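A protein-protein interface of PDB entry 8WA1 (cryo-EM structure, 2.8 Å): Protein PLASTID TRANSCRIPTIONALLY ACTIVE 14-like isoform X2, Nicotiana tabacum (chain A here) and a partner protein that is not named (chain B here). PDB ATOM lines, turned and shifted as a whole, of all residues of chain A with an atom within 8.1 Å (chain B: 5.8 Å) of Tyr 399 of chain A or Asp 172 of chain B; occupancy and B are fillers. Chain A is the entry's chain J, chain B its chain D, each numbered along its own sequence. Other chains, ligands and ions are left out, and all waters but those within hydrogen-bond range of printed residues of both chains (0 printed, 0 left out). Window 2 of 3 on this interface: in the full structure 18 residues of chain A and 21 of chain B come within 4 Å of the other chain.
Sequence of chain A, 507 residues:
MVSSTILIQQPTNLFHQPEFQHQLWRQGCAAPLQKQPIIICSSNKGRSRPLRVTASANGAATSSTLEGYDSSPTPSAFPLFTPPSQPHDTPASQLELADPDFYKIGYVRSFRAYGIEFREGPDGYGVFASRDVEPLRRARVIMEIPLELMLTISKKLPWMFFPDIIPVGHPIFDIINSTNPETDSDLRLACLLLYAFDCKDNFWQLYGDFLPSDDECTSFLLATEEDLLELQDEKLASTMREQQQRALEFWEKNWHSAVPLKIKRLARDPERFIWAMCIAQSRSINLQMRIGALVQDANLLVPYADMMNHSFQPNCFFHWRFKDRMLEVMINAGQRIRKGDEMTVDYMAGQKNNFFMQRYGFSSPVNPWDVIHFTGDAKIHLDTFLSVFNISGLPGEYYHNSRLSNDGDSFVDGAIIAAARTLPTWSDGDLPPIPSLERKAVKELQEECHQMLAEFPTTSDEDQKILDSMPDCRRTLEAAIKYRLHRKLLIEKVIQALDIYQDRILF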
ATOM      1  N   GLN A 313      13.879   2.334   5.041  1.00  0.00           N
ATOM      2  CA  GLN A 313      13.304   2.077   6.359  1.00  0.00           C
ATOM      3  C   GLN A 313      12.094   2.991   6.488  1.00  0.00           C
ATOM      4  O   GLN A 313      12.159   4.047   7.132  1.00  0.00           O
ATOM      5  CB  GLN A 313      14.323   2.310   7.475  1.00  0.00           C
ATOM      6  CG  GLN A 313      15.509   1.357   7.430  1.00  0.00           C
ATOM      7  CD  GLN A 313      16.488   1.579   8.567  1.00  0.00           C
ATOM      8  OE1 GLN A 313      17.431   0.808   8.747  1.00  0.00           O
ATOM      9  NE2 GLN A 313      16.270   2.638   9.339  1.00  0.00           N
ATOM     10  N   LEU A 386      28.217 -12.006   9.133  1.00  0.00           N
ATOM     11  CA  LEU A 386      27.056 -11.426   9.801  1.00  0.00           C
ATOM     12  C   LEU A 386      27.301 -11.274  11.298  1.00  0.00           C
ATOM     13  O   LEU A 386      26.745 -10.373  11.936  1.00  0.00           O
ATOM     14  CB  LEU A 386      25.817 -12.284   9.545  1.00  0.00           C
ATOM     15  CG  LEU A 386      25.435 -12.531   8.082  1.00  0.00           C
ATOM     16  CD1 LEU A 386      24.133 -13.311   7.993  1.00  0.00           C
ATOM     17  CD2 LEU A 386      25.342 -11.225   7.310  1.00  0.00           C
ATOM     18  N   PHE A 389      29.696  -8.247  11.814  1.00  0.00           N
ATOM     19  CA  PHE A 389      28.977  -7.033  11.455  1.00  0.00           C
ATOM     20  C   PHE A 389      27.599  -6.951  12.100  1.00  0.00           C
ATOM     21  O   PHE A 389      26.826  -6.040  11.778  1.00  0.00           O
ATOM     22  CB  PHE A 389      28.872  -6.914   9.938  1.00  0.00           C
ATOM     23  CG  PHE A 389      30.131  -6.424   9.287  1.00  0.00           C
ATOM     24  CD1 PHE A 389      30.490  -5.090   9.372  1.00  0.00           C
ATOM     25  CD2 PHE A 389      30.957  -7.293   8.596  1.00  0.00           C
ATOM     26  CE1 PHE A 389      31.649  -4.631   8.782  1.00  0.00           C
ATOM     27  CE2 PHE A 389      32.119  -6.838   8.004  1.00  0.00           C
ATOM     28  CZ  PHE A 389      32.463  -5.507   8.096  1.00  0.00           C
ATOM     29  N   ASN A 390      27.289  -7.871  13.012  1.00  0.00           N
ATOM     30  CA  ASN A 390      26.063  -7.833  13.812  1.00  0.00           C
ATOM     31  C   ASN A 390      24.819  -7.704  12.936  1.00  0.00           C
ATOM     32  O   ASN A 390      24.007  -6.788  13.092  1.00  0.00           O
ATOM     33  CB  ASN A 390      26.125  -6.708  14.843  1.00  0.00           C
ATOM     34  CG  ASN A 390      27.258  -6.887  15.836  1.00  0.00           C
ATOM     35  OD1 ASN A 390      28.127  -6.026  15.966  1.00  0.00           O
ATOM     36  ND2 ASN A 390      27.256  -8.011  16.540  1.00  0.00           N
ATOM     37  N   ILE A 391      24.673  -8.635  12.000  1.00  0.00           N
ATOM     38  CA  ILE A 391      23.496  -8.729  11.147  1.00  0.00           C
ATOM     39  C   ILE A 391      22.689  -9.938  11.591  1.00  0.00           C
ATOM     40  O   ILE A 391      23.225 -11.048  11.693  1.00  0.00           O
ATOM     41  CB  ILE A 391      23.882  -8.828   9.660  1.00  0.00           C
ATOM     42  CG1 ILE A 391      24.668  -7.585   9.236  1.00  0.00           C
ATOM     43  CG2 ILE A 391      22.642  -8.999   8.798  1.00  0.00           C
ATOM     44  CD1 ILE A 391      25.091  -7.594   7.785  1.00  0.00           C
ATOM     45  N   SER A 392      21.403  -9.724  11.858  1.00  0.00           N
ATOM     46  CA  SER A 392      20.531 -10.766  12.376  1.00  0.00           C
ATOM     47  C   SER A 392      19.283 -10.870  11.513  1.00  0.00           C
ATOM     48  O   SER A 392      18.790  -9.874  10.979  1.00  0.00           O
ATOM     49  CB  SER A 392      20.135 -10.493  13.833  1.00  0.00           C
ATOM     50  OG  SER A 392      19.417  -9.277  13.946  1.00  0.00           O
ATOM     51  N   GLY A 393      18.778 -12.089  11.388  1.00  0.00           N
ATOM     52  CA  GLY A 393      17.586 -12.367  10.618  1.00  0.00           C
ATOM     53  C   GLY A 393      17.864 -13.319   9.472  1.00  0.00           C
ATOM     54  O   GLY A 393      18.998 -13.722   9.215  1.00  0.00           O
ATOM     55  N   LEU A 394      16.789 -13.674   8.781  1.00  0.00           N
ATOM     56  CA  LEU A 394      16.861 -14.578   7.646  1.00  0.00           C
ATOM     57  C   LEU A 394      17.422 -13.846   6.434  1.00  0.00           C
ATOM     58  O   LEU A 394      17.440 -12.614   6.389  1.00  0.00           O
ATOM     59  CB  LEU A 394      15.474 -15.152   7.365  1.00  0.00           C
ATOM     60  CG  LEU A 394      14.855 -15.955   8.512  1.00  0.00           C
ATOM     61  CD1 LEU A 394      13.462 -16.436   8.143  1.00  0.00           C
ATOM     62  CD2 LEU A 394      15.746 -17.126   8.893  1.00  0.00           C
ATOM     63  N   GLY A 396      16.108 -13.224   3.774  1.00  0.00           N
ATOM     64  CA  GLY A 396      15.094 -12.351   3.220  1.00  0.00           C
ATOM     65  C   GLY A 396      14.815 -11.101   4.016  1.00  0.00           C
ATOM     66  O   GLY A 396      14.149 -10.192   3.512  1.00  0.00           O
ATOM     67  N   GLU A 397      15.307 -11.024   5.251  1.00  0.00           N
ATOM     68  CA  GLU A 397      15.113  -9.860   6.109  1.00  0.00           C
ATOM     69  C   GLU A 397      16.370  -9.670   6.945  1.00  0.00           C
ATOM     70  O   GLU A 397      16.605 -10.417   7.899  1.00  0.00           O
ATOM     71  CB  GLU A 397      13.879 -10.031   6.999  1.00  0.00           C
ATOM     72  CG  GLU A 397      13.441  -8.770   7.732  1.00  0.00           C
ATOM     73  CD  GLU A 397      14.170  -8.563   9.046  1.00  0.00           C
ATOM     74  OE1 GLU A 397      14.624  -9.562   9.642  1.00  0.00           O
ATOM     75  OE2 GLU A 397      14.286  -7.399   9.484  1.00  0.00           O
ATOM     76  N   TYR A 398      17.174  -8.671   6.591  1.00  0.00           N
ATOM     77  CA  TYR A 398      18.413  -8.373   7.292  1.00  0.00           C
ATOM     78  C   TYR A 398      18.317  -7.000   7.938  1.00  0.00           C
ATOM     79  O   TYR A 398      17.902  -6.030   7.295  1.00  0.00           O
ATOM     80  CB  TYR A 398      19.620  -8.418   6.346  1.00  0.00           C
ATOM     81  CG  TYR A 398      20.181  -9.801   6.102  1.00  0.00           C
ATOM     82  CD1 TYR A 398      20.048 -10.805   7.052  1.00  0.00           C
ATOM     83  CD2 TYR A 398      20.852 -10.100   4.923  1.00  0.00           C
ATOM     84  CE1 TYR A 398      20.564 -12.069   6.834  1.00  0.00           C
ATOM     85  CE2 TYR A 398      21.371 -11.362   4.696  1.00  0.00           C
ATOM     86  CZ  TYR A 398      21.224 -12.341   5.654  1.00  0.00           C
ATOM     87  OH  TYR A 398      21.738 -13.597   5.433  1.00  0.00           O
ATOM     88  N   TYR A 399      18.695  -6.924   9.211  1.00  0.00           N
ATOM     89  CA  TYR A 399      18.716  -5.656   9.923  1.00  0.00           C
ATOM     90  C   TYR A 399      19.852  -5.677  10.933  1.00  0.00           C
ATOM     91  O   TYR A 399      20.244  -6.733  11.437  1.00  0.00           O
ATOM     92  CB  TYR A 399      17.380  -5.371  10.622  1.00  0.00           C
ATOM     93  CG  TYR A 399      17.120  -6.229  11.840  1.00  0.00           C
ATOM     94  CD1 TYR A 399      16.676  -7.538  11.709  1.00  0.00           C
ATOM     95  CD2 TYR A 399      17.311  -5.726  13.121  1.00  0.00           C
ATOM     96  CE1 TYR A 399      16.436  -8.325  12.820  1.00  0.00           C
ATOM     97  CE2 TYR A 399      17.072  -6.506  14.238  1.00  0.00           C
ATOM     98  CZ  TYR A 399      16.634  -7.804  14.081  1.00  0.00           C
ATOM     99  OH  TYR A 399      16.396  -8.582  15.189  1.00  0.00           O
ATOM    100  N   HIS A 400      20.376  -4.491  11.224  1.00  0.00           N
ATOM    101  CA  HIS A 400      21.442  -4.333  12.202  1.00  0.00           C
ATOM    102  C   HIS A 400      20.845  -4.271  13.601  1.00  0.00           C
ATOM    103  O   HIS A 400      20.080  -3.355  13.918  1.00  0.00           O
ATOM    104  CB  HIS A 400      22.252  -3.071  11.911  1.00  0.00           C
ATOM    105  CG  HIS A 400      21.638  -2.189  10.869  1.00  0.00           C
ATOM    106  ND1 HIS A 400      20.534  -1.401  11.117  1.00  0.00           N
ATOM    107  CD2 HIS A 400      21.968  -1.976   9.573  1.00  0.00           C
ATOM    108  CE1 HIS A 400      20.214  -0.738  10.020  1.00  0.00           C
ATOM    109  NE2 HIS A 400      21.069  -1.069   9.068  1.00  0.00           N
ATOM    110  N   ASN A 401      21.199  -5.247  14.435  1.00  0.00           N
ATOM    111  CA  ASN A 401      20.663  -5.349  15.789  1.00  0.00           C
ATOM    112  C   ASN A 401      21.382  -4.329  16.663  1.00  0.00           C
ATOM    113  O   ASN A 401      22.463  -4.598  17.193  1.00  0.00           O
ATOM    114  CB  ASN A 401      20.826  -6.765  16.329  1.00  0.00           C
ATOM    115  CG  ASN A 401      20.188  -6.947  17.694  1.00  0.00           C
ATOM    116  OD1 ASN A 401      19.352  -6.147  18.114  1.00  0.00           O
ATOM    117  ND2 ASN A 401      20.579  -8.008  18.390  1.00  0.00           N
ATOM    118  N   SER A 402      20.926  -3.097  16.684  1.00  0.00           N
ATOM    119  CA  SER A 402      21.649  -2.054  17.407  1.00  0.00           C
ATOM    120  C   SER A 402      21.545  -2.191  18.906  1.00  0.00           C
ATOM    121  O   SER A 402      22.086  -1.388  19.661  1.00  0.00           O
ATOM    122  CB  SER A 402      21.126  -0.703  16.994  1.00  0.00           C
ATOM    123  OG  SER A 402      19.782  -0.801  16.566  1.00  0.00           O
ATOM    124  N   ARG A 403      20.844  -3.212  19.341  1.00  0.00           N
ATOM    125  CA  ARG A 403      20.683  -3.455  20.746  1.00  0.00           C
ATOM    126  C   ARG A 403      21.876  -4.212  21.196  1.00  0.00           C
ATOM    127  O   ARG A 403      22.284  -4.108  22.340  1.00  0.00           O
ATOM    128  CB  ARG A 403      19.419  -4.261  20.963  1.00  0.00           C
ATOM    129  N   LEU A 404      22.458  -4.982  20.299  1.00  0.00           N
ATOM    130  CA  LEU A 404      23.631  -5.763  20.608  1.00  0.00           C
ATOM    131  C   LEU A 404      24.744  -4.898  20.192  1.00  0.00           C
ATOM    132  O   LEU A 404      25.870  -5.080  20.614  1.00  0.00           O
ATOM    133  CB  LEU A 404      23.663  -7.014  19.738  1.00  0.00           C
ATOM    134  CG  LEU A 404      23.828  -8.348  20.453  1.00  0.00           C
ATOM    135  CD1 LEU A 404      25.227  -8.893  20.219  1.00  0.00           C
ATOM    136  CD2 LEU A 404      23.544  -8.198  21.938  1.00  0.00           C
ATOM    137  N   VAL A 412      27.961  -0.027  10.072  1.00  0.00           N
ATOM    138  CA  VAL A 412      26.945  -0.929   9.547  1.00  0.00           C
ATOM    139  C   VAL A 412      25.773  -0.118   9.010  1.00  0.00           C
ATOM    140  O   VAL A 412      25.288   0.818   9.661  1.00  0.00           O
ATOM    141  CB  VAL A 412      26.502  -1.928  10.627  1.00  0.00           C
ATOM    142  CG1 VAL A 412      26.070  -1.202  11.896  1.00  0.00           C
ATOM    143  CG2 VAL A 412      25.385  -2.819  10.104  1.00  0.00           C
ATOM    144  N   ASP A 413      25.319  -0.469   7.815  1.00  0.00           N
ATOM    145  CA  ASP A 413      24.218   0.210   7.137  1.00  0.00           C
ATOM    146  C   ASP A 413      23.750  -0.699   6.004  1.00  0.00           C
ATOM    147  O   ASP A 413      24.157  -1.864   5.915  1.00  0.00           O
ATOM    148  CB  ASP A 413      24.637   1.596   6.640  1.00  0.00           C
ATOM    149  CG  ASP A 413      25.709   1.534   5.570  1.00  0.00           C
ATOM    150  OD1 ASP A 413      26.536   0.601   5.606  1.00  0.00           O
ATOM    151  OD2 ASP A 413      25.726   2.422   4.693  1.00  0.00           O
ATOM    152  N   ILE A 417      24.883  -4.656   4.184  1.00  0.00           N
ATOM    153  CA  ILE A 417      23.861  -5.679   3.983  1.00  0.00           C
ATOM    154  C   ILE A 417      23.823  -6.113   2.523  1.00  0.00           C
ATOM    155  O   ILE A 417      23.803  -7.313   2.213  1.00  0.00           O
ATOM    156  CB  ILE A 417      22.491  -5.163   4.459  1.00  0.00           C
ATOM    157  CG1 ILE A 417      22.522  -4.882   5.962  1.00  0.00           C
ATOM    158  CG2 ILE A 417      21.397  -6.161   4.115  1.00  0.00           C
ATOM    159  CD1 ILE A 417      21.208  -4.385   6.518  1.00  0.00           C
ATOM    160  N   ARG A 421      24.813  -9.746   0.921  1.00  0.00           N
ATOM    161  CA  ARG A 421      23.895 -10.416   0.008  1.00  0.00           C
ATOM    162  C   ARG A 421      24.578 -10.769  -1.309  1.00  0.00           C
ATOM    163  O   ARG A 421      24.354 -11.851  -1.864  1.00  0.00           O
ATOM    164  CB  ARG A 421      22.664  -9.542  -0.231  1.00  0.00           C
ATOM    165  CG  ARG A 421      21.710  -9.521   0.949  1.00  0.00           C
ATOM    166  CD  ARG A 421      20.565  -8.545   0.751  1.00  0.00           C
ATOM    167  NE  ARG A 421      19.656  -8.570   1.892  1.00  0.00           N
ATOM    168  CZ  ARG A 421      18.681  -7.692   2.095  1.00  0.00           C
ATOM    169  NH1 ARG A 421      18.482  -6.705   1.233  1.00  0.00           N
ATOM    170  NH2 ARG A 421      17.905  -7.799   3.164  1.00  0.00           N
ATOM    171  N   HIS B 140      26.609 -15.786  18.269  1.00  0.00           N
ATOM    172  CA  HIS B 140      25.357 -16.381  17.814  1.00  0.00           C
ATOM    173  C   HIS B 140      25.590 -17.763  17.213  1.00  0.00           C
ATOM    174  O   HIS B 140      24.720 -18.637  17.297  1.00  0.00           O
ATOM    175  CB  HIS B 140      24.678 -15.460  16.799  1.00  0.00           C
ATOM    176  CG  HIS B 140      23.340 -15.949  16.341  1.00  0.00           C
ATOM    177  ND1 HIS B 140      23.182 -16.773  15.248  1.00  0.00           N
ATOM    178  CD2 HIS B 140      22.096 -15.729  16.829  1.00  0.00           C
ATOM    179  CE1 HIS B 140      21.899 -17.040  15.082  1.00  0.00           C
ATOM    180  NE2 HIS B 140      21.219 -16.419  16.028  1.00  0.00           N
ATOM    181  N   MET B 166      19.710 -16.753  24.944  1.00  0.00           N
ATOM    182  CA  MET B 166      19.934 -15.882  23.796  1.00  0.00           C
ATOM    183  C   MET B 166      19.058 -14.640  23.845  1.00  0.00           C
ATOM    184  O   MET B 166      19.511 -13.556  23.463  1.00  0.00           O
ATOM    185  CB  MET B 166      19.664 -16.632  22.491  1.00  0.00           C
ATOM    186  CG  MET B 166      20.581 -17.807  22.222  1.00  0.00           C
ATOM    187  SD  MET B 166      20.099 -18.692  20.726  1.00  0.00           S
ATOM    188  CE  MET B 166      20.223 -17.383  19.510  1.00  0.00           C
ATOM    189  N   GLU B 167      17.815 -14.779  24.308  1.00  0.00           N
ATOM    190  CA  GLU B 167      16.896 -13.650  24.361  1.00  0.00           C
ATOM    191  C   GLU B 167      17.309 -12.638  25.423  1.00  0.00           C
ATOM    192  O   GLU B 167      17.232 -11.427  25.188  1.00  0.00           O
ATOM    193  CB  GLU B 167      15.473 -14.149  24.623  1.00  0.00           C
ATOM    194  CG  GLU B 167      14.434 -13.045  24.748  1.00  0.00           C
ATOM    195  CD  GLU B 167      14.254 -12.260  23.464  1.00  0.00           C
ATOM    196  OE1 GLU B 167      14.506 -12.823  22.377  1.00  0.00           O
ATOM    197  OE2 GLU B 167      13.864 -11.076  23.541  1.00  0.00           O
ATOM    198  N   LYS B 170      19.918 -10.316  24.280  1.00  0.00           N
ATOM    199  CA  LYS B 170      19.421  -9.422  23.232  1.00  0.00           C
ATOM    200  C   LYS B 170      19.606 -10.006  21.835  1.00  0.00           C
ATOM    201  O   LYS B 170      19.409  -9.280  20.856  1.00  0.00           O
ATOM    202  CB  LYS B 170      20.065  -8.022  23.276  1.00  0.00           C
ATOM    203  CG  LYS B 170      19.871  -7.300  24.598  1.00  0.00           C
ATOM    204  CD  LYS B 170      18.398  -7.193  24.954  1.00  0.00           C
ATOM    205  CE  LYS B 170      18.202  -6.528  26.307  1.00  0.00           C
ATOM    206  NZ  LYS B 170      16.765  -6.439  26.680  1.00  0.00           N
ATOM    207  N   TYR B 171      19.979 -11.276  21.707  1.00  0.00           N
ATOM    208  CA  TYR B 171      20.083 -11.886  20.389  1.00  0.00           C
ATOM    209  C   TYR B 171      18.700 -12.198  19.830  1.00  0.00           C
ATOM    210  O   TYR B 171      17.739 -12.418  20.572  1.00  0.00           O
ATOM    211  CB  TYR B 171      20.920 -13.164  20.449  1.00  0.00           C
ATOM    212  CG  TYR B 171      22.411 -12.930  20.546  1.00  0.00           C
ATOM    213  CD1 TYR B 171      23.163 -12.638  19.415  1.00  0.00           C
ATOM    214  CD2 TYR B 171      23.068 -13.007  21.766  1.00  0.00           C
ATOM    215  CE1 TYR B 171      24.527 -12.425  19.497  1.00  0.00           C
ATOM    216  CE2 TYR B 171      24.431 -12.797  21.858  1.00  0.00           C
ATOM    217  CZ  TYR B 171      25.155 -12.507  20.722  1.00  0.00           C
ATOM    218  OH  TYR B 171      26.513 -12.297  20.812  1.00  0.00           O
ATOM    219  N   ASP B 172      18.605 -12.217  18.503  1.00  0.00           N
ATOM    220  CA  ASP B 172      17.362 -12.603  17.851  1.00  0.00           C
ATOM    221  C   ASP B 172      17.243 -14.121  17.828  1.00  0.00           C
ATOM    222  O   ASP B 172      18.173 -14.828  17.431  1.00  0.00           O
ATOM    223  CB  ASP B 172      17.306 -12.039  16.432  1.00  0.00           C
ATOM    224  CG  ASP B 172      15.907 -12.063  15.850  1.00  0.00           C
ATOM    225  OD1 ASP B 172      15.067 -11.247  16.285  1.00  0.00           O
ATOM    226  OD2 ASP B 172      15.647 -12.896  14.958  1.00  0.00           O
ATOM    227  N   ILE B 173      16.083 -14.624  18.253  1.00  0.00           N
ATOM    228  CA  ILE B 173      15.899 -16.049  18.492  1.00  0.00           C
ATOM    229  C   ILE B 173      14.995 -16.699  17.449  1.00  0.00           C
ATOM    230  O   ILE B 173      14.569 -17.842  17.634  1.00  0.00           O
ATOM    231  CB  ILE B 173      15.360 -16.301  19.908  1.00  0.00           C
ATOM    232  CG1 ILE B 173      13.991 -15.640  20.080  1.00  0.00           C
ATOM    233  CG2 ILE B 173      16.336 -15.778  20.951  1.00  0.00           C
ATOM    234  CD1 ILE B 173      13.408 -15.795  21.466  1.00  0.00           C
ATOM    235  N   ARG B 174      14.691 -15.999  16.354  1.00  0.00           N
ATOM    236  CA  ARG B 174      13.815 -16.572  15.334  1.00  0.00           C
ATOM    237  C   ARG B 174      14.512 -17.699  14.579  1.00  0.00           C
ATOM    238  O   ARG B 174      13.979 -18.810  14.464  1.00  0.00           O
ATOM    239  CB  ARG B 174      13.352 -15.483  14.367  1.00  0.00           C
ATOM    240  CG  ARG B 174      12.490 -16.002  13.228  1.00  0.00           C
ATOM    241  CD  ARG B 174      12.127 -14.893  12.254  1.00  0.00           C
ATOM    242  NE  ARG B 174      11.344 -15.395  11.128  1.00  0.00           N
ATOM    243  CZ  ARG B 174      10.923 -14.642  10.117  1.00  0.00           C
ATOM    244  NH1 ARG B 174      11.208 -13.348  10.087  1.00  0.00           N
ATOM    245  NH2 ARG B 174      10.216 -15.183   9.134  1.00  0.00           N
ATOM    246  N   GLN B 175      15.710 -17.426  14.054  1.00  0.00           N
ATOM    247  CA  GLN B 175      16.430 -18.431  13.279  1.00  0.00           C
ATOM    248  C   GLN B 175      16.802 -19.632  14.138  1.00  0.00           C
ATOM    249  O   GLN B 175      16.709 -20.779  13.686  1.00  0.00           O
ATOM    250  CB  GLN B 175      17.678 -17.808  12.653  1.00  0.00           C
ATOM    251  CG  GLN B 175      18.506 -18.768  11.817  1.00  0.00           C
ATOM    252  CD  GLN B 175      19.766 -18.124  11.272  1.00  0.00           C
ATOM    253  OE1 GLN B 175      20.573 -18.776  10.609  1.00  0.00           O
ATOM    254  NE2 GLN B 175      19.940 -16.837  11.548  1.00  0.00           N
ATOM    255  N   ALA B 176      17.227 -19.389  15.380  1.00  0.00           N
ATOM    256  CA  ALA B 176      17.576 -20.491  16.266  1.00  0.00           C
ATOM    257  C   ALA B 176      16.356 -21.344  16.592  1.00  0.00           C
ATOM    258  O   ALA B 176      16.447 -22.575  16.644  1.00  0.00           O
ATOM    259  CB  ALA B 176      18.218 -19.955  17.544  1.00  0.00           C
ATOM    260  N   ARG B 206       7.551 -15.452  14.084  1.00  0.00           N
ATOM    261  CA  ARG B 206       7.012 -15.934  12.823  1.00  0.00           C
ATOM    262  C   ARG B 206       7.848 -17.107  12.328  1.00  0.00           C
ATOM    263  O   ARG B 206       9.005 -17.282  12.720  1.00  0.00           O
ATOM    264  CB  ARG B 206       6.988 -14.819  11.770  1.00  0.00           C
ATOM    265  CG  ARG B 206       6.220 -13.581  12.204  1.00  0.00           C
ATOM    266  CD  ARG B 206       6.927 -12.311  11.762  1.00  0.00           C
ATOM    267  NE  ARG B 206       8.298 -12.259  12.262  1.00  0.00           N
ATOM    268  CZ  ARG B 206       8.639 -11.814  13.467  1.00  0.00           C
ATOM    269  NH1 ARG B 206       7.706 -11.381  14.304  1.00  0.00           N
ATOM    270  NH2 ARG B 206       9.912 -11.803  13.837  1.00  0.00           N
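Of the 21 printed residues of chain A, 4 touch a printed residue of chain B.
Hydrophobic or aromatic side chains of chain A that line the printed part of chain B: Leu 394, Tyr 399 and Leu 404.
Along chain A the printed residues that touch a printed residue of chain B span positions 394 to 404.
Of the 11 printed residues of chain B, 4 touch a printed residue of chain A.
Printed residues of chain B that touch a printed residue of chain A: Lys 170, Tyr 171, Asp 172 and Arg 174.
Among the printed residues, no Asp or Glu carboxylate lies within 4 Å of a Lys or Arg side-chain nitrogen of the other chain.
Leu 394 of chain A touches Arg 174 of chain B.
Lys 170 of chain B touches Leu 404 of chain A.
CD1 of Leu 404 of chain A touches CZ of Tyr 171 of chain B, 3.6 Å away.
The backbone carbonyl oxygen (O) of Lys 170 of chain B sits at hydrogen-bond distance from the side-chain amide nitrogen (ND2) of Asn 401 of chain A (3.0 Å).
The side-chain carboxylate (OD1) of Asp 172 of chain B is in hydrogen-bond range of the side-chain hydroxyl (OH) of Tyr 399 of chain A (3.2 Å).
Tyr 399 of chain A touches just one residue of chain B: Asp 172.
Of chain A, only Tyr 399 comes within 4 Å of Asp 172 of chain B.
Of the printed residues of chain A, Lys 170 of chain B touches Asn 401 and Leu 404.
Of the printed residues of chain A, Arg 174 of chain B touches Leu 394.
Printed residues of chain B within 4 Å of Leu 404 of chain A: Lys 170 and Tyr 171.
Of the printed residues of chain B, Asn 401 of chain A touches Lys 170.
Glu 167 of chain B touches none of the printed residues of chain A.
Ile 173 of chain B touches none of the printed residues of chain A.
The nearest printed residue of chain B that does not touch Tyr 399 of chain A is Tyr 171 of chain B (6.3 Å).
The backbone NH (N) of Asn 401 of chain A sits at hydrogen-bond distance from the backbone carbonyl oxygen (O) of Asn 390 of chain A (3.5 Å).
N of Tyr 171 of chain B lies within hydrogen-bond range of O of Met 166 of chain B (2.9 Å).
The guanidinium group of Arg 174 of chain B sits at hydrogen-bond distance from the backbone carbonyl oxygen of Arg 206 of chain B (3.4 Å).
The backbone NH (N) of Ser 392 of chain A sits at hydrogen-bond distance from the backbone carbonyl oxygen (O) of Tyr 399 of chain A, at 3.2 Å.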
